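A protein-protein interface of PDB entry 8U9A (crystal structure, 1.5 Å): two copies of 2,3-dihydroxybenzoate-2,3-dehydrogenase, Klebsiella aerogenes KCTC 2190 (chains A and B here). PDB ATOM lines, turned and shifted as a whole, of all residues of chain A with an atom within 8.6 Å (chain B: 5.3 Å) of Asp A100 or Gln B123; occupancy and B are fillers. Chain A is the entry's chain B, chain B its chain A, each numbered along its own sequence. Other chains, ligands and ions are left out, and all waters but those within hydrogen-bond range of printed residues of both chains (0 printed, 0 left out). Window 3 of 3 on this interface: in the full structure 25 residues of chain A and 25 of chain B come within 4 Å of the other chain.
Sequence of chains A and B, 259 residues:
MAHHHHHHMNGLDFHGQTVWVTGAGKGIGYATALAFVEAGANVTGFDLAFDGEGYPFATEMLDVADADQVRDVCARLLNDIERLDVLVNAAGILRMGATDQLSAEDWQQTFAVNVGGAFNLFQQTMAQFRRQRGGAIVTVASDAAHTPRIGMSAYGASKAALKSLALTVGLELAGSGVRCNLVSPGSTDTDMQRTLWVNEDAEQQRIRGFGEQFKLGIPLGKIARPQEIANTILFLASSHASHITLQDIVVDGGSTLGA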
ATOM      1  N   GLY A  97      34.377 -12.567   2.731  1.00  0.00           N
ATOM      2  CA  GLY A  97      34.811 -12.092   1.436  1.00  0.00           C
ATOM      3  C   GLY A  97      33.968 -10.931   0.979  1.00  0.00           C
ATOM      4  O   GLY A  97      32.837 -10.738   1.430  1.00  0.00           O
ATOM      5  N   ALA A  98      34.546 -10.138   0.083  1.00  0.00           N
ATOM      6  CA  ALA A  98      33.755  -9.139  -0.621  1.00  0.00           C
ATOM      7  C   ALA A  98      32.593  -9.831  -1.324  1.00  0.00           C
ATOM      8  O   ALA A  98      32.737 -10.943  -1.837  1.00  0.00           O
ATOM      9  CB  ALA A  98      34.618  -8.399  -1.636  1.00  0.00           C
ATOM     10  N   THR A  99      31.436  -9.160  -1.374  1.00  0.00           N
ATOM     11  CA  THR A  99      30.249  -9.807  -1.918  1.00  0.00           C
ATOM     12  C   THR A  99      30.496 -10.346  -3.321  1.00  0.00           C
ATOM     13  O   THR A  99      30.069 -11.465  -3.639  1.00  0.00           O
ATOM     14  CB  THR A  99      29.075  -8.841  -1.937  1.00  0.00           C
ATOM     15  OG1 THR A  99      28.764  -8.466  -0.595  1.00  0.00           O
ATOM     16  CG2 THR A  99      27.844  -9.508  -2.547  1.00  0.00           C
ATOM     17  N   ASP A 100      31.191  -9.584  -4.161  1.00  0.00           N
ATOM     18  CA  ASP A 100      31.382  -9.992  -5.550  1.00  0.00           C
ATOM     19  C   ASP A 100      32.571 -10.925  -5.741  1.00  0.00           C
ATOM     20  O   ASP A 100      32.826 -11.340  -6.878  1.00  0.00           O
ATOM     21  CB  ASP A 100      31.508  -8.774  -6.488  1.00  0.00           C
ATOM     22  CG  ASP A 100      32.622  -7.821  -6.111  1.00  0.00           C
ATOM     23  OD1 ASP A 100      32.910  -7.639  -4.907  1.00  0.00           O
ATOM     24  OD2 ASP A 100      33.176  -7.197  -7.041  1.00  0.00           O
ATOM     25  N   GLN A 101      33.296 -11.260  -4.664  1.00  0.00           N
ATOM     26  CA  GLN A 101      34.390 -12.225  -4.713  1.00  0.00           C
ATOM     27  C   GLN A 101      34.053 -13.555  -4.054  1.00  0.00           C
ATOM     28  O   GLN A 101      34.781 -14.532  -4.261  1.00  0.00           O
ATOM     29  CB  GLN A 101      35.643 -11.652  -4.035  1.00  0.00           C
ATOM     30  CG  GLN A 101      36.205 -10.397  -4.699  1.00  0.00           C
ATOM     31  CD  GLN A 101      37.525  -9.941  -4.093  1.00  0.00           C
ATOM     32  OE1 GLN A 101      38.219 -10.715  -3.433  1.00  0.00           O
ATOM     33  NE2 GLN A 101      37.867  -8.676  -4.303  1.00  0.00           N
ATOM     34  N   LEU A 102      32.977 -13.619  -3.276  1.00  0.00           N
ATOM     35  CA  LEU A 102      32.639 -14.835  -2.554  1.00  0.00           C
ATOM     36  C   LEU A 102      32.333 -15.968  -3.520  1.00  0.00           C
ATOM     37  O   LEU A 102      31.592 -15.793  -4.491  1.00  0.00           O
ATOM     38  CB  LEU A 102      31.423 -14.582  -1.665  1.00  0.00           C
ATOM     39  CG  LEU A 102      31.211 -15.637  -0.587  1.00  0.00           C
ATOM     40  CD1 LEU A 102      32.292 -15.533   0.488  1.00  0.00           C
ATOM     41  CD2 LEU A 102      29.818 -15.470   0.023  1.00  0.00           C
ATOM     42  N   SER A 103      32.882 -17.147  -3.237  1.00  0.00           N
ATOM     43  CA  SER A 103      32.647 -18.290  -4.100  1.00  0.00           C
ATOM     44  C   SER A 103      31.234 -18.836  -3.937  1.00  0.00           C
ATOM     45  O   SER A 103      30.572 -18.672  -2.906  1.00  0.00           O
ATOM     46  CB  SER A 103      33.649 -19.405  -3.808  1.00  0.00           C
ATOM     47  OG  SER A 103      33.402 -19.984  -2.546  1.00  0.00           O
ATOM     48  N   ALA A 104      30.786 -19.531  -4.979  1.00  0.00           N
ATOM     49  CA  ALA A 104      29.485 -20.184  -4.933  1.00  0.00           C
ATOM     50  C   ALA A 104      29.421 -21.183  -3.789  1.00  0.00           C
ATOM     51  O   ALA A 104      28.422 -21.244  -3.062  1.00  0.00           O
ATOM     52  CB  ALA A 104      29.215 -20.878  -6.272  1.00  0.00           C
ATOM     53  N   GLU A 105      30.483 -21.959  -3.596  1.00  0.00           N
ATOM     54  CA  GLU A 105      30.480 -22.933  -2.512  1.00  0.00           C
ATOM     55  C   GLU A 105      30.358 -22.260  -1.157  1.00  0.00           C
ATOM     56  O   GLU A 105      29.620 -22.737  -0.291  1.00  0.00           O
ATOM     57  CB  GLU A 105      31.742 -23.789  -2.555  1.00  0.00           C
ATOM     58  CG  GLU A 105      31.716 -24.901  -1.542  1.00  0.00           C
ATOM     59  CD  GLU A 105      32.817 -25.917  -1.774  1.00  0.00           C
ATOM     60  OE1 GLU A 105      33.999 -25.510  -1.803  1.00  0.00           O
ATOM     61  OE2 GLU A 105      32.499 -27.116  -1.941  1.00  0.00           O
ATOM     62  N   TRP A 107      28.972 -19.314  -0.475  1.00  0.00           N
ATOM     63  CA  TRP A 107      27.590 -18.843  -0.348  1.00  0.00           C
ATOM     64  C   TRP A 107      26.652 -19.972   0.046  1.00  0.00           C
ATOM     65  O   TRP A 107      25.882 -19.854   1.008  1.00  0.00           O
ATOM     66  CB  TRP A 107      27.150 -18.215  -1.676  1.00  0.00           C
ATOM     67  CG  TRP A 107      25.736 -17.765  -1.680  1.00  0.00           C
ATOM     68  CD1 TRP A 107      24.664 -18.427  -2.206  1.00  0.00           C
ATOM     69  CD2 TRP A 107      25.226 -16.554  -1.118  1.00  0.00           C
ATOM     70  NE1 TRP A 107      23.516 -17.704  -2.009  1.00  0.00           N
ATOM     71  CE2 TRP A 107      23.836 -16.544  -1.346  1.00  0.00           C
ATOM     72  CE3 TRP A 107      25.810 -15.473  -0.446  1.00  0.00           C
ATOM     73  CZ2 TRP A 107      23.025 -15.503  -0.926  1.00  0.00           C
ATOM     74  CZ3 TRP A 107      24.995 -14.436  -0.041  1.00  0.00           C
ATOM     75  CH2 TRP A 107      23.633 -14.452  -0.275  1.00  0.00           C
ATOM     76  N   SER A 153      29.129 -10.007   4.212  1.00  0.00           N
ATOM     77  CA  SER A 153      27.772  -9.841   3.711  1.00  0.00           C
ATOM     78  C   SER A 153      26.991 -11.154   3.779  1.00  0.00           C
ATOM     79  O   SER A 153      25.846 -11.168   4.233  1.00  0.00           O
ATOM     80  CB  SER A 153      27.782  -9.283   2.283  1.00  0.00           C
ATOM     81  OG  SER A 153      28.386 -10.200   1.376  1.00  0.00           O
ATOM     82  N   ALA A 154      27.591 -12.269   3.341  1.00  0.00           N
ATOM     83  CA  ALA A 154      26.860 -13.533   3.336  1.00  0.00           C
ATOM     84  C   ALA A 154      26.681 -14.070   4.750  1.00  0.00           C
ATOM     85  O   ALA A 154      25.598 -14.537   5.111  1.00  0.00           O
ATOM     86  CB  ALA A 154      27.586 -14.567   2.478  1.00  0.00           C
ATOM     87  N   ALA B 118      19.284 -11.846  -5.931  1.00  0.00           N
ATOM     88  CA  ALA B 118      19.958 -10.572  -5.685  1.00  0.00           C
ATOM     89  C   ALA B 118      21.457 -10.770  -5.498  1.00  0.00           C
ATOM     90  O   ALA B 118      22.253  -9.972  -5.990  1.00  0.00           O
ATOM     91  CB  ALA B 118      19.341  -9.880  -4.475  1.00  0.00           C
ATOM     92  N   PHE B 119      21.869 -11.821  -4.779  1.00  0.00           N
ATOM     93  CA  PHE B 119      23.295 -12.100  -4.650  1.00  0.00           C
ATOM     94  C   PHE B 119      23.957 -12.205  -6.025  1.00  0.00           C
ATOM     95  O   PHE B 119      25.005 -11.605  -6.269  1.00  0.00           O
ATOM     96  CB  PHE B 119      23.498 -13.382  -3.838  1.00  0.00           C
ATOM     97  CG  PHE B 119      24.914 -13.899  -3.819  1.00  0.00           C
ATOM     98  CD1 PHE B 119      25.924 -13.182  -3.180  1.00  0.00           C
ATOM     99  CD2 PHE B 119      25.243 -15.093  -4.438  1.00  0.00           C
ATOM    100  CE1 PHE B 119      27.203 -13.674  -3.129  1.00  0.00           C
ATOM    101  CE2 PHE B 119      26.535 -15.600  -4.397  1.00  0.00           C
ATOM    102  CZ  PHE B 119      27.532 -14.869  -3.753  1.00  0.00           C
ATOM    103  N   ASN B 120      23.353 -12.969  -6.942  1.00  0.00           N
ATOM    104  CA  ASN B 120      23.940 -13.130  -8.264  1.00  0.00           C
ATOM    105  C   ASN B 120      23.987 -11.800  -9.005  1.00  0.00           C
ATOM    106  O   ASN B 120      24.996 -11.471  -9.645  1.00  0.00           O
ATOM    107  CB  ASN B 120      23.147 -14.166  -9.055  1.00  0.00           C
ATOM    108  CG  ASN B 120      23.253 -15.555  -8.456  1.00  0.00           C
ATOM    109  OD1 ASN B 120      24.228 -15.875  -7.770  1.00  0.00           O
ATOM    110  ND2 ASN B 120      22.251 -16.387  -8.708  1.00  0.00           N
ATOM    111  N   LEU B 121      22.900 -11.024  -8.947  1.00  0.00           N
ATOM    112  CA  LEU B 121      22.921  -9.717  -9.604  1.00  0.00           C
ATOM    113  C   LEU B 121      24.004  -8.825  -9.017  1.00  0.00           C
ATOM    114  O   LEU B 121      24.723  -8.148  -9.756  1.00  0.00           O
ATOM    115  CB  LEU B 121      21.559  -9.033  -9.478  1.00  0.00           C
ATOM    116  CG  LEU B 121      20.605  -9.221 -10.657  1.00  0.00           C
ATOM    117  CD1 LEU B 121      21.175  -8.606 -11.937  1.00  0.00           C
ATOM    118  CD2 LEU B 121      20.273 -10.672 -10.862  1.00  0.00           C
ATOM    119  N   PHE B 122      24.133  -8.801  -7.686  1.00  0.00           N
ATOM    120  CA  PHE B 122      25.193  -8.007  -7.082  1.00  0.00           C
ATOM    121  C   PHE B 122      26.571  -8.474  -7.536  1.00  0.00           C
ATOM    122  O   PHE B 122      27.435  -7.651  -7.873  1.00  0.00           O
ATOM    123  CB  PHE B 122      25.097  -8.079  -5.556  1.00  0.00           C
ATOM    124  CG  PHE B 122      23.921  -7.370  -4.973  1.00  0.00           C
ATOM    125  CD1 PHE B 122      23.522  -6.144  -5.454  1.00  0.00           C
ATOM    126  CD2 PHE B 122      23.240  -7.909  -3.880  1.00  0.00           C
ATOM    127  CE1 PHE B 122      22.459  -5.469  -4.854  1.00  0.00           C
ATOM    128  CE2 PHE B 122      22.176  -7.229  -3.302  1.00  0.00           C
ATOM    129  CZ  PHE B 122      21.789  -6.018  -3.793  1.00  0.00           C
ATOM    130  N   GLN B 123      26.805  -9.789  -7.564  1.00  0.00           N
ATOM    131  CA  GLN B 123      28.097 -10.286  -8.024  1.00  0.00           C
ATOM    132  C   GLN B 123      28.408  -9.831  -9.437  1.00  0.00           C
ATOM    133  O   GLN B 123      29.576  -9.589  -9.777  1.00  0.00           O
ATOM    134  CB  GLN B 123      28.135 -11.807  -7.955  1.00  0.00           C
ATOM    135  CG  GLN B 123      28.172 -12.336  -6.521  1.00  0.00           C
ATOM    136  CD  GLN B 123      29.057 -13.553  -6.416  1.00  0.00           C
ATOM    137  OE1 GLN B 123      28.928 -14.522  -7.192  1.00  0.00           O
ATOM    138  NE2 GLN B 123      30.031 -13.497  -5.508  1.00  0.00           N
ATOM    139  N   GLN B 124      27.391  -9.720 -10.284  1.00  0.00           N
ATOM    140  CA  GLN B 124      27.652  -9.346 -11.662  1.00  0.00           C
ATOM    141  C   GLN B 124      27.612  -7.848 -11.921  1.00  0.00           C
ATOM    142  O   GLN B 124      28.036  -7.437 -13.006  1.00  0.00           O
ATOM    143  CB  GLN B 124      26.652 -10.037 -12.601  1.00  0.00           C
ATOM    144  CG  GLN B 124      26.742 -11.550 -12.554  1.00  0.00           C
ATOM    145  CD  GLN B 124      28.151 -12.074 -12.701  1.00  0.00           C
ATOM    146  OE1 GLN B 124      28.925 -11.599 -13.524  1.00  0.00           O
ATOM    147  NE2 GLN B 124      28.477 -13.091 -11.921  1.00  0.00           N
ATOM    148  N   THR B 125      27.107  -7.024 -10.999  1.00  0.00           N
ATOM    149  CA  THR B 125      27.005  -5.596 -11.258  1.00  0.00           C
ATOM    150  C   THR B 125      27.865  -4.728 -10.366  1.00  0.00           C
ATOM    151  O   THR B 125      28.060  -3.556 -10.693  1.00  0.00           O
ATOM    152  CB  THR B 125      25.558  -5.094 -11.117  1.00  0.00           C
ATOM    153  OG1 THR B 125      25.051  -5.358  -9.802  1.00  0.00           O
ATOM    154  CG2 THR B 125      24.675  -5.751 -12.175  1.00  0.00           C
ATOM    155  N   MET B 126      28.421  -5.249  -9.277  1.00  0.00           N
ATOM    156  CA  MET B 126      29.152  -4.358  -8.376  1.00  0.00           C
ATOM    157  C   MET B 126      30.345  -3.707  -9.062  1.00  0.00           C
ATOM    158  O   MET B 126      30.614  -2.525  -8.830  1.00  0.00           O
ATOM    159  CB  MET B 126      29.583  -5.124  -7.128  1.00  0.00           C
ATOM    160  CG  MET B 126      28.433  -5.272  -6.150  1.00  0.00           C
ATOM    161  SD  MET B 126      28.836  -6.292  -4.726  1.00  0.00           S
ATOM    162  CE  MET B 126      29.827  -5.128  -3.803  1.00  0.00           C
ATOM    163  N   ALA B 127      31.060  -4.437  -9.920  1.00  0.00           N
ATOM    164  CA  ALA B 127      32.197  -3.841 -10.619  1.00  0.00           C
ATOM    165  C   ALA B 127      31.763  -2.690 -11.519  1.00  0.00           C
ATOM    166  O   ALA B 127      32.475  -1.687 -11.627  1.00  0.00           O
ATOM    167  CB  ALA B 127      32.944  -4.901 -11.426  1.00  0.00           C
ATOM    168  N   ARG B 130      31.078   0.353  -9.334  1.00  0.00           N
ATOM    169  CA  ARG B 130      32.335   0.960  -8.892  1.00  0.00           C
ATOM    170  C   ARG B 130      33.000   1.742 -10.019  1.00  0.00           C
ATOM    171  O   ARG B 130      33.482   2.863  -9.815  1.00  0.00           O
ATOM    172  CB  ARG B 130      33.296  -0.106  -8.375  1.00  0.00           C
ATOM    173  CG  ARG B 130      32.903  -0.719  -7.054  1.00  0.00           C
ATOM    174  CD  ARG B 130      34.087  -1.527  -6.504  1.00  0.00           C
ATOM    175  NE  ARG B 130      33.657  -2.556  -5.566  1.00  0.00           N
ATOM    176  CZ  ARG B 130      33.462  -3.831  -5.878  1.00  0.00           C
ATOM    177  NH1 ARG B 130      33.721  -4.300  -7.092  1.00  0.00           N
ATOM    178  NH2 ARG B 130      33.011  -4.661  -4.944  1.00  0.00           N
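No position is printed for both chains.
The side-chain amide nitrogen of Gln B123 lies within hydrogen-bond range of the backbone carbonyl oxygen of Leu A102, 3.0 Å away. O of Thr A99 sits at hydrogen-bond distance from NE2 of Gln B123 (2.8 Å). NH1 of Arg B130 is in salt-bridge range of OD2 of Asp A100, 2.9 Å away.
Printed residues of chain B that touch a printed residue of chain A: Phe B119, Gln B123, Met B126 and Arg B130. Hydrophobic or aromatic side chains of chain B within 4 Å of the printed part of chain A: Phe B119 and Met B126. Of the 12 printed residues of chain A, 4 touch a printed residue of chain B. Hydrophobic or aromatic side chains of chain A within 4 Å of the printed part of chain B: Trp A107. Among the printed residues, 7 pairs touch across the chains.
The side-chain hydroxyl of Ser A153 lies within hydrogen-bond range of the side-chain hydroxyl of Thr A99 (2.7 Å).
CE1 of Phe B119 touches O of Thr A99 (3.7 Å). Met B126 touches Thr A99 (SD to CB, 3.8 Å). Asp A100 touches Gln B123. Phe B119 touches Trp A107.
Printed residues of chain B within 4 Å of Leu A102: Gln B123. Ala B118 touches none of the printed residues of chain A. Gln B123 touches just these residues of chain A: Thr A99 (2.8 Å), Asp A100 (3.6 Å) and Leu A102 (3.0 Å). Printed residues of chain A within 4 Å of Met B126: Thr A99 (3.8 Å). Ala B127 touches none of the printed residues of chain A. Of the printed residues of chain A, Arg B130 touches Asp A100 (2.9 Å). The nearest residue of chain B that does not touch Asp A100 is Met B126 (4.1 Å). The nearest printed residue of chain A that does not touch Gln B123 is Gln A101 (4.05 Å).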
